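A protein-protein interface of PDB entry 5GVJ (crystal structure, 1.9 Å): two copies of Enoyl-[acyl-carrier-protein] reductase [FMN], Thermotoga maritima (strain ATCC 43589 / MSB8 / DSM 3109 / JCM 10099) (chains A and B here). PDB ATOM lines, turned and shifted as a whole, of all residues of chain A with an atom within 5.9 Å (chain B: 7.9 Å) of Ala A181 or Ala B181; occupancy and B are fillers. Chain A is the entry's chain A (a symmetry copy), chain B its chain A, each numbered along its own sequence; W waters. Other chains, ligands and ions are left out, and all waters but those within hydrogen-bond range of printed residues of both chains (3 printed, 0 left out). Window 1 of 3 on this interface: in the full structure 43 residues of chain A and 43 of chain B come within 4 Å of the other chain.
Of the 24 printed residues of chain B, 13 touch a printed residue of chain A. Hydrophobic or aromatic side chains of chain B that line the printed part of chain A: Phe B153, Ile B173, Ala B181, Ala B184, Leu B185 and Leu B308. Along chain B the printed residues that touch a printed residue of chain A span positions 152 to 308. Of the 13 printed residues of chain A, 10 touch a printed residue of chain B.
Water W3 lies within hydrogen-bond range of the backbone carbonyl oxygen of Ala B184 and the guanidinium group of Arg A177. Water W2 bridges O of Ala A184 (2.9 Å) and NE of Arg B177 (3.4 Å). Water W1 lies within hydrogen-bond range of N of Phe B153 (3.1 Å) and N of Phe A153 (3.1 Å).
Arg A177 touches Leu B185, and with the chains exchanged Leu A185 touches Arg B177. Arg A177 touches Gly B186, and with the chains exchanged Gly A186 touches Arg B177. Ala A181 touches its own counterpart, Ala B181. Ala A184 touches Thr B304, and with the chains exchanged Thr A304 touches Ala B184. Of the 27 pairs that touch across the chains among the printed residues, 22 have their exchanged pair printed and touching as well.
Gly A176 touches none of the printed residues of chain B. Ala A180 touches none of the printed residues of chain B. Ala A182 touches just one residue of chain B: Phe B153 (3.9 Å). Ala B181 touches four residues of chain A. Printed residues of chain A within 4 Å of Ala B182: Phe A153. Of the printed residues of chain A, Gly B186 touches Arg A177. The nearest residue of chain B that does not touch Ala A181 is Ala B180 (5.5 Å). The nearest residue of chain A that does not touch Ala B181 is Ala A180 (5.5 Å).
The guanidinium group (NH1) of Arg B177 sits at hydrogen-bond distance from the backbone carbonyl oxygen (O) of Leu A185 (2.9 Å). The backbone carbonyl oxygen (O) of Leu B185 lies within hydrogen-bond range of the guanidinium group (NH1) of Arg A177, at 2.9 Å.
Ile B173 touches Phe A153 (CG1 to CE2, 3.5 Å). Phe A153 touches Gly B178 (CZ to O, 3.4 Å). OD1 of Asn B157 touches CD of Arg A177, at 3.9 Å. Ala A181 touches Phe B153 (CB to CZ, 3.8 Å). Leu B185 touches Ala A181 (CD2 to CB, 3.5 Å). Leu B308 touches Phe A183 (CD2 to CB, 3.6 Å). N of Ala A184 touches CD2 of Leu B308, 3.8 Å away. Leu A185 touches Phe B153 (CD1 to CE1, 3.97 Å). CD2 of Leu A185 touches CB of Ala B181, 3.5 Å away. NH1 of Arg B177 touches CA of Gly A186, 3.7 Å away.
The side-chain carboxylate (OD1) of Asp B175 sits close to the backbone NH (N) of Arg B177, 3.4 Å away. The backbone NH (N) of Gly B178 sits at hydrogen-bond distance from the side-chain carboxylate (OD1) of Asp B175 (2.9 Å). O of Ala B182 is in hydrogen-bond range of N of Ala B187 (3.0 Å).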
ATOM      1  N   PHE A 153      -3.347  27.198 -31.668  1.00  0.00           N
ATOM      2  CA  PHE A 153      -3.503  26.035 -30.809  1.00  0.00           C
ATOM      3  C   PHE A 153      -2.186  25.648 -30.169  1.00  0.00           C
ATOM      4  O   PHE A 153      -2.136  25.304 -28.982  1.00  0.00           O
ATOM      5  CB  PHE A 153      -4.055  24.865 -31.622  1.00  0.00           C
ATOM      6  CG  PHE A 153      -4.837  23.903 -30.812  1.00  0.00           C
ATOM      7  CD1 PHE A 153      -6.200  24.075 -30.652  1.00  0.00           C
ATOM      8  CD2 PHE A 153      -4.210  22.849 -30.178  1.00  0.00           C
ATOM      9  CE1 PHE A 153      -6.926  23.200 -29.878  1.00  0.00           C
ATOM     10  CE2 PHE A 153      -4.929  21.966 -29.413  1.00  0.00           C
ATOM     11  CZ  PHE A 153      -6.294  22.144 -29.263  1.00  0.00           C
ATOM     12  N   GLY A 176     -17.475  32.474 -27.928  1.00  0.00           N
ATOM     13  CA  GLY A 176     -17.223  32.060 -26.557  1.00  0.00           C
ATOM     14  C   GLY A 176     -16.537  30.711 -26.459  1.00  0.00           C
ATOM     15  O   GLY A 176     -15.740  30.483 -25.541  1.00  0.00           O
ATOM     16  N   ARG A 177     -16.844  29.798 -27.384  1.00  0.00           N
ATOM     17  CA  ARG A 177     -16.091  28.544 -27.481  1.00  0.00           C
ATOM     18  C   ARG A 177     -14.602  28.808 -27.607  1.00  0.00           C
ATOM     19  O   ARG A 177     -13.785  28.190 -26.918  1.00  0.00           O
ATOM     20  CB  ARG A 177     -16.558  27.745 -28.697  1.00  0.00           C
ATOM     21  CG  ARG A 177     -17.656  26.787 -28.425  1.00  0.00           C
ATOM     22  CD  ARG A 177     -17.805  25.867 -29.605  1.00  0.00           C
ATOM     23  NE  ARG A 177     -19.179  25.406 -29.738  1.00  0.00           N
ATOM     24  CZ  ARG A 177     -19.550  24.402 -30.521  1.00  0.00           C
ATOM     25  NH1 ARG A 177     -18.645  23.753 -31.247  1.00  0.00           N
ATOM     26  NH2 ARG A 177     -20.826  24.050 -30.575  1.00  0.00           N
ATOM     27  N   GLY A 178     -14.231  29.706 -28.517  1.00  0.00           N
ATOM     28  CA  GLY A 178     -12.827  30.014 -28.705  1.00  0.00           C
ATOM     29  C   GLY A 178     -12.202  30.641 -27.474  1.00  0.00           C
ATOM     30  O   GLY A 178     -11.033  30.392 -27.164  1.00  0.00           O
ATOM     31  N   MET A 179     -12.971  31.460 -26.752  1.00  0.00           N
ATOM     32  CA  MET A 179     -12.462  32.033 -25.515  1.00  0.00           C
ATOM     33  C   MET A 179     -12.145  30.933 -24.513  1.00  0.00           C
ATOM     34  O   MET A 179     -11.088  30.950 -23.873  1.00  0.00           O
ATOM     35  CB  MET A 179     -13.465  33.028 -24.927  1.00  0.00           C
ATOM     36  CG  MET A 179     -12.986  33.666 -23.641  1.00  0.00           C
ATOM     37  SD  MET A 179     -14.060  35.017 -23.054  1.00  0.00           S
ATOM     38  CE  MET A 179     -13.937  34.777 -21.291  1.00  0.00           C
ATOM     39  N   ALA A 180     -13.046  29.956 -24.379  1.00  0.00           N
ATOM     40  CA  ALA A 180     -12.801  28.864 -23.442  1.00  0.00           C
ATOM     41  C   ALA A 180     -11.618  28.017 -23.894  1.00  0.00           C
ATOM     42  O   ALA A 180     -10.758  27.659 -23.081  1.00  0.00           O
ATOM     43  CB  ALA A 180     -14.057  28.005 -23.282  1.00  0.00           C
ATOM     44  N   ALA A 181     -11.549  27.711 -25.191  1.00  0.00           N
ATOM     45  CA  ALA A 181     -10.414  26.972 -25.731  1.00  0.00           C
ATOM     46  C   ALA A 181      -9.099  27.695 -25.480  1.00  0.00           C
ATOM     47  O   ALA A 181      -8.111  27.071 -25.085  1.00  0.00           O
ATOM     48  CB  ALA A 181     -10.611  26.751 -27.225  1.00  0.00           C
ATOM     49  N   ALA A 182      -9.061  29.016 -25.715  1.00  0.00           N
ATOM     50  CA  ALA A 182      -7.841  29.777 -25.462  1.00  0.00           C
ATOM     51  C   ALA A 182      -7.450  29.713 -23.994  1.00  0.00           C
ATOM     52  O   ALA A 182      -6.272  29.536 -23.660  1.00  0.00           O
ATOM     53  CB  ALA A 182      -8.021  31.232 -25.901  1.00  0.00           C
ATOM     54  N   PHE A 183      -8.428  29.855 -23.102  1.00  0.00           N
ATOM     55  CA  PHE A 183      -8.143  29.787 -21.673  1.00  0.00           C
ATOM     56  C   PHE A 183      -7.629  28.406 -21.281  1.00  0.00           C
ATOM     57  O   PHE A 183      -6.733  28.278 -20.431  1.00  0.00           O
ATOM     58  CB  PHE A 183      -9.410  30.153 -20.892  1.00  0.00           C
ATOM     59  CG  PHE A 183      -9.643  31.642 -20.772  1.00  0.00           C
ATOM     60  CD1 PHE A 183      -9.331  32.498 -21.817  1.00  0.00           C
ATOM     61  CD2 PHE A 183     -10.174  32.177 -19.611  1.00  0.00           C
ATOM     62  CE1 PHE A 183      -9.536  33.869 -21.704  1.00  0.00           C
ATOM     63  CE2 PHE A 183     -10.393  33.546 -19.495  1.00  0.00           C
ATOM     64  CZ  PHE A 183     -10.072  34.384 -20.545  1.00  0.00           C
ATOM     65  N   ALA A 184      -8.167  27.357 -21.909  1.00  0.00           N
ATOM     66  CA  ALA A 184      -7.671  26.008 -21.657  1.00  0.00           C
ATOM     67  C   ALA A 184      -6.204  25.871 -22.046  1.00  0.00           C
ATOM     68  O   ALA A 184      -5.435  25.191 -21.360  1.00  0.00           O
ATOM     69  CB  ALA A 184      -8.515  24.983 -22.416  1.00  0.00           C
ATOM     70  N   LEU A 185      -5.798  26.488 -23.161  1.00  0.00           N
ATOM     71  CA  LEU A 185      -4.400  26.426 -23.565  1.00  0.00           C
ATOM     72  C   LEU A 185      -3.491  27.252 -22.658  1.00  0.00           C
ATOM     73  O   LEU A 185      -2.265  27.129 -22.766  1.00  0.00           O
ATOM     74  CB  LEU A 185      -4.248  26.898 -25.012  1.00  0.00           C
ATOM     75  CG  LEU A 185      -4.982  26.087 -26.081  1.00  0.00           C
ATOM     76  CD1 LEU A 185      -4.952  26.781 -27.439  1.00  0.00           C
ATOM     77  CD2 LEU A 185      -4.383  24.687 -26.170  1.00  0.00           C
ATOM     78  N   GLY A 186      -4.052  28.083 -21.783  1.00  0.00           N
ATOM     79  CA  GLY A 186      -3.274  28.892 -20.856  1.00  0.00           C
ATOM     80  C   GLY A 186      -3.467  30.397 -20.976  1.00  0.00           C
ATOM     81  O   GLY A 186      -2.875  31.142 -20.179  1.00  0.00           O
ATOM     82  N   THR A 304     -19.816  26.761 -22.315  1.00  0.00           N
ATOM     83  CA  THR A 304     -18.755  25.835 -22.689  1.00  0.00           C
ATOM     84  C   THR A 304     -18.070  25.258 -21.454  1.00  0.00           C
ATOM     85  O   THR A 304     -17.816  24.047 -21.388  1.00  0.00           O
ATOM     86  CB  THR A 304     -17.745  26.533 -23.602  1.00  0.00           C
ATOM     87  OG1 THR A 304     -18.426  27.010 -24.765  1.00  0.00           O
ATOM     88  CG2 THR A 304     -16.638  25.554 -24.048  1.00  0.00           C
ATOM     89  N   THR B 152      -6.392  24.070 -36.590  1.00  0.00           N
ATOM     90  CA  THR B 152      -7.248  23.317 -35.673  1.00  0.00           C
ATOM     91  C   THR B 152      -8.215  24.231 -34.940  1.00  0.00           C
ATOM     92  O   THR B 152      -9.401  23.906 -34.794  1.00  0.00           O
ATOM     93  CB  THR B 152      -6.383  22.551 -34.672  1.00  0.00           C
ATOM     94  OG1 THR B 152      -5.574  21.617 -35.381  1.00  0.00           O
ATOM     95  CG2 THR B 152      -7.241  21.788 -33.659  1.00  0.00           C
ATOM     96  N   PHE B 153      -7.718  25.375 -34.465  1.00  0.00           N
ATOM     97  CA  PHE B 153      -8.525  26.256 -33.634  1.00  0.00           C
ATOM     98  C   PHE B 153      -9.803  26.655 -34.342  1.00  0.00           C
ATOM     99  O   PHE B 153     -10.878  26.699 -33.731  1.00  0.00           O
ATOM    100  CB  PHE B 153      -7.718  27.502 -33.269  1.00  0.00           C
ATOM    101  CG  PHE B 153      -8.129  28.113 -31.985  1.00  0.00           C
ATOM    102  CD1 PHE B 153      -7.531  27.717 -30.802  1.00  0.00           C
ATOM    103  CD2 PHE B 153      -9.138  29.055 -31.950  1.00  0.00           C
ATOM    104  CE1 PHE B 153      -7.930  28.262 -29.604  1.00  0.00           C
ATOM    105  CE2 PHE B 153      -9.533  29.612 -30.760  1.00  0.00           C
ATOM    106  CZ  PHE B 153      -8.925  29.212 -29.581  1.00  0.00           C
ATOM    107  N   VAL B 156     -11.962  22.840 -35.975  1.00  0.00           N
ATOM    108  CA  VAL B 156     -12.761  22.049 -35.045  1.00  0.00           C
ATOM    109  C   VAL B 156     -14.036  22.792 -34.666  1.00  0.00           C
ATOM    110  O   VAL B 156     -15.108  22.191 -34.556  1.00  0.00           O
ATOM    111  CB  VAL B 156     -11.933  21.679 -33.800  1.00  0.00           C
ATOM    112  CG1 VAL B 156     -12.808  20.982 -32.758  1.00  0.00           C
ATOM    113  CG2 VAL B 156     -10.770  20.796 -34.195  1.00  0.00           C
ATOM    114  N   ASN B 157     -13.934  24.109 -34.453  1.00  0.00           N
ATOM    115  CA  ASN B 157     -15.099  24.909 -34.090  1.00  0.00           C
ATOM    116  C   ASN B 157     -16.149  24.855 -35.190  1.00  0.00           C
ATOM    117  O   ASN B 157     -17.316  24.543 -34.932  1.00  0.00           O
ATOM    118  CB  ASN B 157     -14.649  26.349 -33.818  1.00  0.00           C
ATOM    119  CG  ASN B 157     -15.768  27.241 -33.279  1.00  0.00           C
ATOM    120  OD1 ASN B 157     -16.941  26.866 -33.271  1.00  0.00           O
ATOM    121  ND2 ASN B 157     -15.390  28.434 -32.807  1.00  0.00           N
ATOM    122  N   ALA B 169     -10.634  15.954 -32.916  1.00  0.00           N
ATOM    123  CA  ALA B 169      -9.688  17.005 -33.273  1.00  0.00           C
ATOM    124  C   ALA B 169      -8.302  16.403 -33.465  1.00  0.00           C
ATOM    125  O   ALA B 169      -7.865  15.593 -32.647  1.00  0.00           O
ATOM    126  CB  ALA B 169      -9.639  18.076 -32.189  1.00  0.00           C
ATOM    127  N   ILE B 173      -2.141  18.782 -30.961  1.00  0.00           N
ATOM    128  CA  ILE B 173      -2.579  18.292 -29.666  1.00  0.00           C
ATOM    129  C   ILE B 173      -1.535  17.319 -29.149  1.00  0.00           C
ATOM    130  O   ILE B 173      -1.300  16.272 -29.759  1.00  0.00           O
ATOM    131  CB  ILE B 173      -3.959  17.630 -29.753  1.00  0.00           C
ATOM    132  CG1 ILE B 173      -4.953  18.603 -30.396  1.00  0.00           C
ATOM    133  CG2 ILE B 173      -4.424  17.245 -28.359  1.00  0.00           C
ATOM    134  CD1 ILE B 173      -6.153  17.937 -30.988  1.00  0.00           C
ATOM    135  N   ASP B 175      -1.060  17.220 -25.293  1.00  0.00           N
ATOM    136  CA  ASP B 175      -1.134  17.222 -23.836  1.00  0.00           C
ATOM    137  C   ASP B 175      -2.580  17.436 -23.395  1.00  0.00           C
ATOM    138  O   ASP B 175      -3.484  17.637 -24.216  1.00  0.00           O
ATOM    139  CB  ASP B 175      -0.193  18.273 -23.232  1.00  0.00           C
ATOM    140  CG  ASP B 175      -0.429  19.663 -23.791  1.00  0.00           C
ATOM    141  OD1 ASP B 175      -1.580  19.962 -24.191  1.00  0.00           O
ATOM    142  OD2 ASP B 175       0.536  20.451 -23.824  1.00  0.00           O
ATOM    143  N   GLY B 176      -2.784  17.404 -22.072  1.00  0.00           N
ATOM    144  CA  GLY B 176      -4.129  17.498 -21.527  1.00  0.00           C
ATOM    145  C   GLY B 176      -4.758  18.863 -21.725  1.00  0.00           C
ATOM    146  O   GLY B 176      -5.978  18.968 -21.901  1.00  0.00           O
ATOM    147  N   ARG B 177      -3.947  19.924 -21.684  1.00  0.00           N
ATOM    148  CA  ARG B 177      -4.433  21.257 -22.054  1.00  0.00           C
ATOM    149  C   ARG B 177      -5.063  21.244 -23.435  1.00  0.00           C
ATOM    150  O   ARG B 177      -6.157  21.782 -23.641  1.00  0.00           O
ATOM    151  CB  ARG B 177      -3.279  22.257 -22.046  1.00  0.00           C
ATOM    152  CG  ARG B 177      -3.073  22.954 -20.753  1.00  0.00           C
ATOM    153  CD  ARG B 177      -2.130  24.106 -20.965  1.00  0.00           C
ATOM    154  NE  ARG B 177      -1.369  24.388 -19.757  1.00  0.00           N
ATOM    155  CZ  ARG B 177      -0.657  25.492 -19.571  1.00  0.00           C
ATOM    156  NH1 ARG B 177      -0.608  26.420 -20.521  1.00  0.00           N
ATOM    157  NH2 ARG B 177       0.001  25.663 -18.435  1.00  0.00           N
ATOM    158  N   GLY B 178      -4.364  20.660 -24.405  1.00  0.00           N
ATOM    159  CA  GLY B 178      -4.891  20.609 -25.754  1.00  0.00           C
ATOM    160  C   GLY B 178      -6.165  19.791 -25.846  1.00  0.00           C
ATOM    161  O   GLY B 178      -7.069  20.118 -26.622  1.00  0.00           O
ATOM    162  N   MET B 179      -6.258  18.720 -25.055  1.00  0.00           N
ATOM    163  CA  MET B 179      -7.485  17.937 -25.034  1.00  0.00           C
ATOM    164  C   MET B 179      -8.649  18.788 -24.550  1.00  0.00           C
ATOM    165  O   MET B 179      -9.735  18.763 -25.138  1.00  0.00           O
ATOM    166  CB  MET B 179      -7.319  16.697 -24.153  1.00  0.00           C
ATOM    167  CG  MET B 179      -8.562  15.835 -24.099  1.00  0.00           C
ATOM    168  SD  MET B 179      -8.308  14.243 -23.247  1.00  0.00           S
ATOM    169  CE  MET B 179      -9.891  14.054 -22.448  1.00  0.00           C
ATOM    170  N   ALA B 180      -8.431  19.566 -23.485  1.00  0.00           N
ATOM    171  CA  ALA B 180      -9.502  20.415 -22.974  1.00  0.00           C
ATOM    172  C   ALA B 180      -9.855  21.506 -23.977  1.00  0.00           C
ATOM    173  O   ALA B 180     -11.037  21.769 -24.224  1.00  0.00           O
ATOM    174  CB  ALA B 180      -9.105  21.022 -21.627  1.00  0.00           C
ATOM    175  N   ALA B 181      -8.841  22.128 -24.580  1.00  0.00           N
ATOM    176  CA  ALA B 181      -9.080  23.131 -25.612  1.00  0.00           C
ATOM    177  C   ALA B 181      -9.873  22.561 -26.779  1.00  0.00           C
ATOM    178  O   ALA B 181     -10.807  23.201 -27.269  1.00  0.00           O
ATOM    179  CB  ALA B 181      -7.750  23.684 -26.107  1.00  0.00           C
ATOM    180  N   ALA B 182      -9.509  21.358 -27.250  1.00  0.00           N
ATOM    181  CA  ALA B 182     -10.249  20.737 -28.345  1.00  0.00           C
ATOM    182  C   ALA B 182     -11.698  20.491 -27.956  1.00  0.00           C
ATOM    183  O   ALA B 182     -12.617  20.744 -28.746  1.00  0.00           O
ATOM    184  CB  ALA B 182      -9.581  19.425 -28.763  1.00  0.00           C
ATOM    185  N   PHE B 183     -11.921  19.997 -26.741  1.00  0.00           N
ATOM    186  CA  PHE B 183     -13.284  19.749 -26.281  1.00  0.00           C
ATOM    187  C   PHE B 183     -14.076  21.048 -26.185  1.00  0.00           C
ATOM    188  O   PHE B 183     -15.275  21.088 -26.501  1.00  0.00           O
ATOM    189  CB  PHE B 183     -13.232  19.027 -24.930  1.00  0.00           C
ATOM    190  CG  PHE B 183     -13.002  17.537 -25.043  1.00  0.00           C
ATOM    191  CD1 PHE B 183     -12.163  17.019 -26.018  1.00  0.00           C
ATOM    192  CD2 PHE B 183     -13.629  16.663 -24.173  1.00  0.00           C
ATOM    193  CE1 PHE B 183     -11.959  15.647 -26.129  1.00  0.00           C
ATOM    194  CE2 PHE B 183     -13.420  15.291 -24.271  1.00  0.00           C
ATOM    195  CZ  PHE B 183     -12.585  14.791 -25.251  1.00  0.00           C
ATOM    196  N   ALA B 184     -13.414  22.134 -25.773  1.00  0.00           N
ATOM    197  CA  ALA B 184     -14.075  23.434 -25.737  1.00  0.00           C
ATOM    198  C   ALA B 184     -14.528  23.868 -27.125  1.00  0.00           C
ATOM    199  O   ALA B 184     -15.602  24.459 -27.277  1.00  0.00           O
ATOM    200  CB  ALA B 184     -13.140  24.486 -25.135  1.00  0.00           C
ATOM    201  N   LEU B 185     -13.713  23.609 -28.153  1.00  0.00           N
ATOM    202  CA  LEU B 185     -14.108  23.965 -29.510  1.00  0.00           C
ATOM    203  C   LEU B 185     -15.229  23.078 -30.045  1.00  0.00           C
ATOM    204  O   LEU B 185     -15.792  23.395 -31.100  1.00  0.00           O
ATOM    205  CB  LEU B 185     -12.901  23.892 -30.446  1.00  0.00           C
ATOM    206  CG  LEU B 185     -11.733  24.830 -30.139  1.00  0.00           C
ATOM    207  CD1 LEU B 185     -10.507  24.505 -30.985  1.00  0.00           C
ATOM    208  CD2 LEU B 185     -12.167  26.279 -30.340  1.00  0.00           C
ATOM    209  N   GLY B 186     -15.557  21.985 -29.359  1.00  0.00           N
ATOM    210  CA  GLY B 186     -16.628  21.091 -29.771  1.00  0.00           C
ATOM    211  C   GLY B 186     -16.215  19.651 -30.038  1.00  0.00           C
ATOM    212  O   GLY B 186     -17.089  18.823 -30.339  1.00  0.00           O
ATOM    213  N   ALA B 187     -14.927  19.307 -29.980  1.00  0.00           N
ATOM    214  CA  ALA B 187     -14.526  17.924 -30.196  1.00  0.00           C
ATOM    215  C   ALA B 187     -14.923  17.055 -29.009  1.00  0.00           C
ATOM    216  O   ALA B 187     -15.082  17.533 -27.886  1.00  0.00           O
ATOM    217  CB  ALA B 187     -13.017  17.826 -30.422  1.00  0.00           C
ATOM    218  N   VAL B 190      -9.578  13.321 -29.239  1.00  0.00           N
ATOM    219  CA  VAL B 190      -8.421  13.945 -29.867  1.00  0.00           C
ATOM    220  C   VAL B 190      -7.539  12.864 -30.470  1.00  0.00           C
ATOM    221  O   VAL B 190      -7.469  11.742 -29.969  1.00  0.00           O
ATOM    222  CB  VAL B 190      -7.606  14.816 -28.880  1.00  0.00           C
ATOM    223  CG1 VAL B 190      -8.416  16.057 -28.466  1.00  0.00           C
ATOM    224  CG2 VAL B 190      -7.190  14.012 -27.652  1.00  0.00           C
ATOM    225  N   PHE B 301      -5.931  17.216 -18.316  1.00  0.00           N
ATOM    226  CA  PHE B 301      -7.262  17.574 -18.800  1.00  0.00           C
ATOM    227  C   PHE B 301      -8.166  17.953 -17.633  1.00  0.00           C
ATOM    228  O   PHE B 301      -8.809  19.010 -17.644  1.00  0.00           O
ATOM    229  CB  PHE B 301      -7.858  16.410 -19.598  1.00  0.00           C
ATOM    230  CG  PHE B 301      -9.322  16.580 -19.914  1.00  0.00           C
ATOM    231  CD1 PHE B 301      -9.725  17.261 -21.051  1.00  0.00           C
ATOM    232  CD2 PHE B 301     -10.295  16.066 -19.067  1.00  0.00           C
ATOM    233  CE1 PHE B 301     -11.079  17.416 -21.346  1.00  0.00           C
ATOM    234  CE2 PHE B 301     -11.634  16.222 -19.350  1.00  0.00           C
ATOM    235  CZ  PHE B 301     -12.027  16.906 -20.486  1.00  0.00           C
ATOM    236  N   THR B 304      -7.102  21.165 -16.004  1.00  0.00           N
ATOM    237  CA  THR B 304      -7.469  22.294 -16.848  1.00  0.00           C
ATOM    238  C   THR B 304      -8.946  22.639 -16.691  1.00  0.00           C
ATOM    239  O   THR B 304      -9.305  23.819 -16.575  1.00  0.00           O
ATOM    240  CB  THR B 304      -7.126  21.993 -18.309  1.00  0.00           C
ATOM    241  OG1 THR B 304      -5.725  21.727 -18.408  1.00  0.00           O
ATOM    242  CG2 THR B 304      -7.463  23.197 -19.213  1.00  0.00           C
ATOM    243  N   VAL B 305      -9.818  21.623 -16.664  1.00  0.00           N
ATOM    244  CA  VAL B 305     -11.254  21.883 -16.530  1.00  0.00           C
ATOM    245  C   VAL B 305     -11.562  22.505 -15.173  1.00  0.00           C
ATOM    246  O   VAL B 305     -12.375  23.438 -15.070  1.00  0.00           O
ATOM    247  CB  VAL B 305     -12.059  20.590 -16.762  1.00  0.00           C
ATOM    248  CG1 VAL B 305     -13.524  20.796 -16.405  1.00  0.00           C
ATOM    249  CG2 VAL B 305     -11.949  20.155 -18.204  1.00  0.00           C
ATOM    250  N   LEU B 308     -10.659  26.120 -15.467  1.00  0.00           N
ATOM    251  CA  LEU B 308     -11.693  26.886 -16.165  1.00  0.00           C
ATOM    252  C   LEU B 308     -12.907  27.112 -15.279  1.00  0.00           C
ATOM    253  O   LEU B 308     -13.538  28.177 -15.329  1.00  0.00           O
ATOM    254  CB  LEU B 308     -12.117  26.167 -17.445  1.00  0.00           C
ATOM    255  CG  LEU B 308     -11.052  26.058 -18.534  1.00  0.00           C
ATOM    256  CD1 LEU B 308     -11.580  25.275 -19.727  1.00  0.00           C
ATOM    257  CD2 LEU B 308     -10.633  27.432 -18.963  1.00  0.00           C
HETATM  258  O   HOH W   1      -4.783  26.505 -34.381  1.00  0.00           O
HETATM  259  O   HOH W   2      -4.259  25.993 -18.799  1.00  0.00           O
HETATM  260  O   HOH W   3     -18.258  23.224 -27.241  1.00  0.00           O
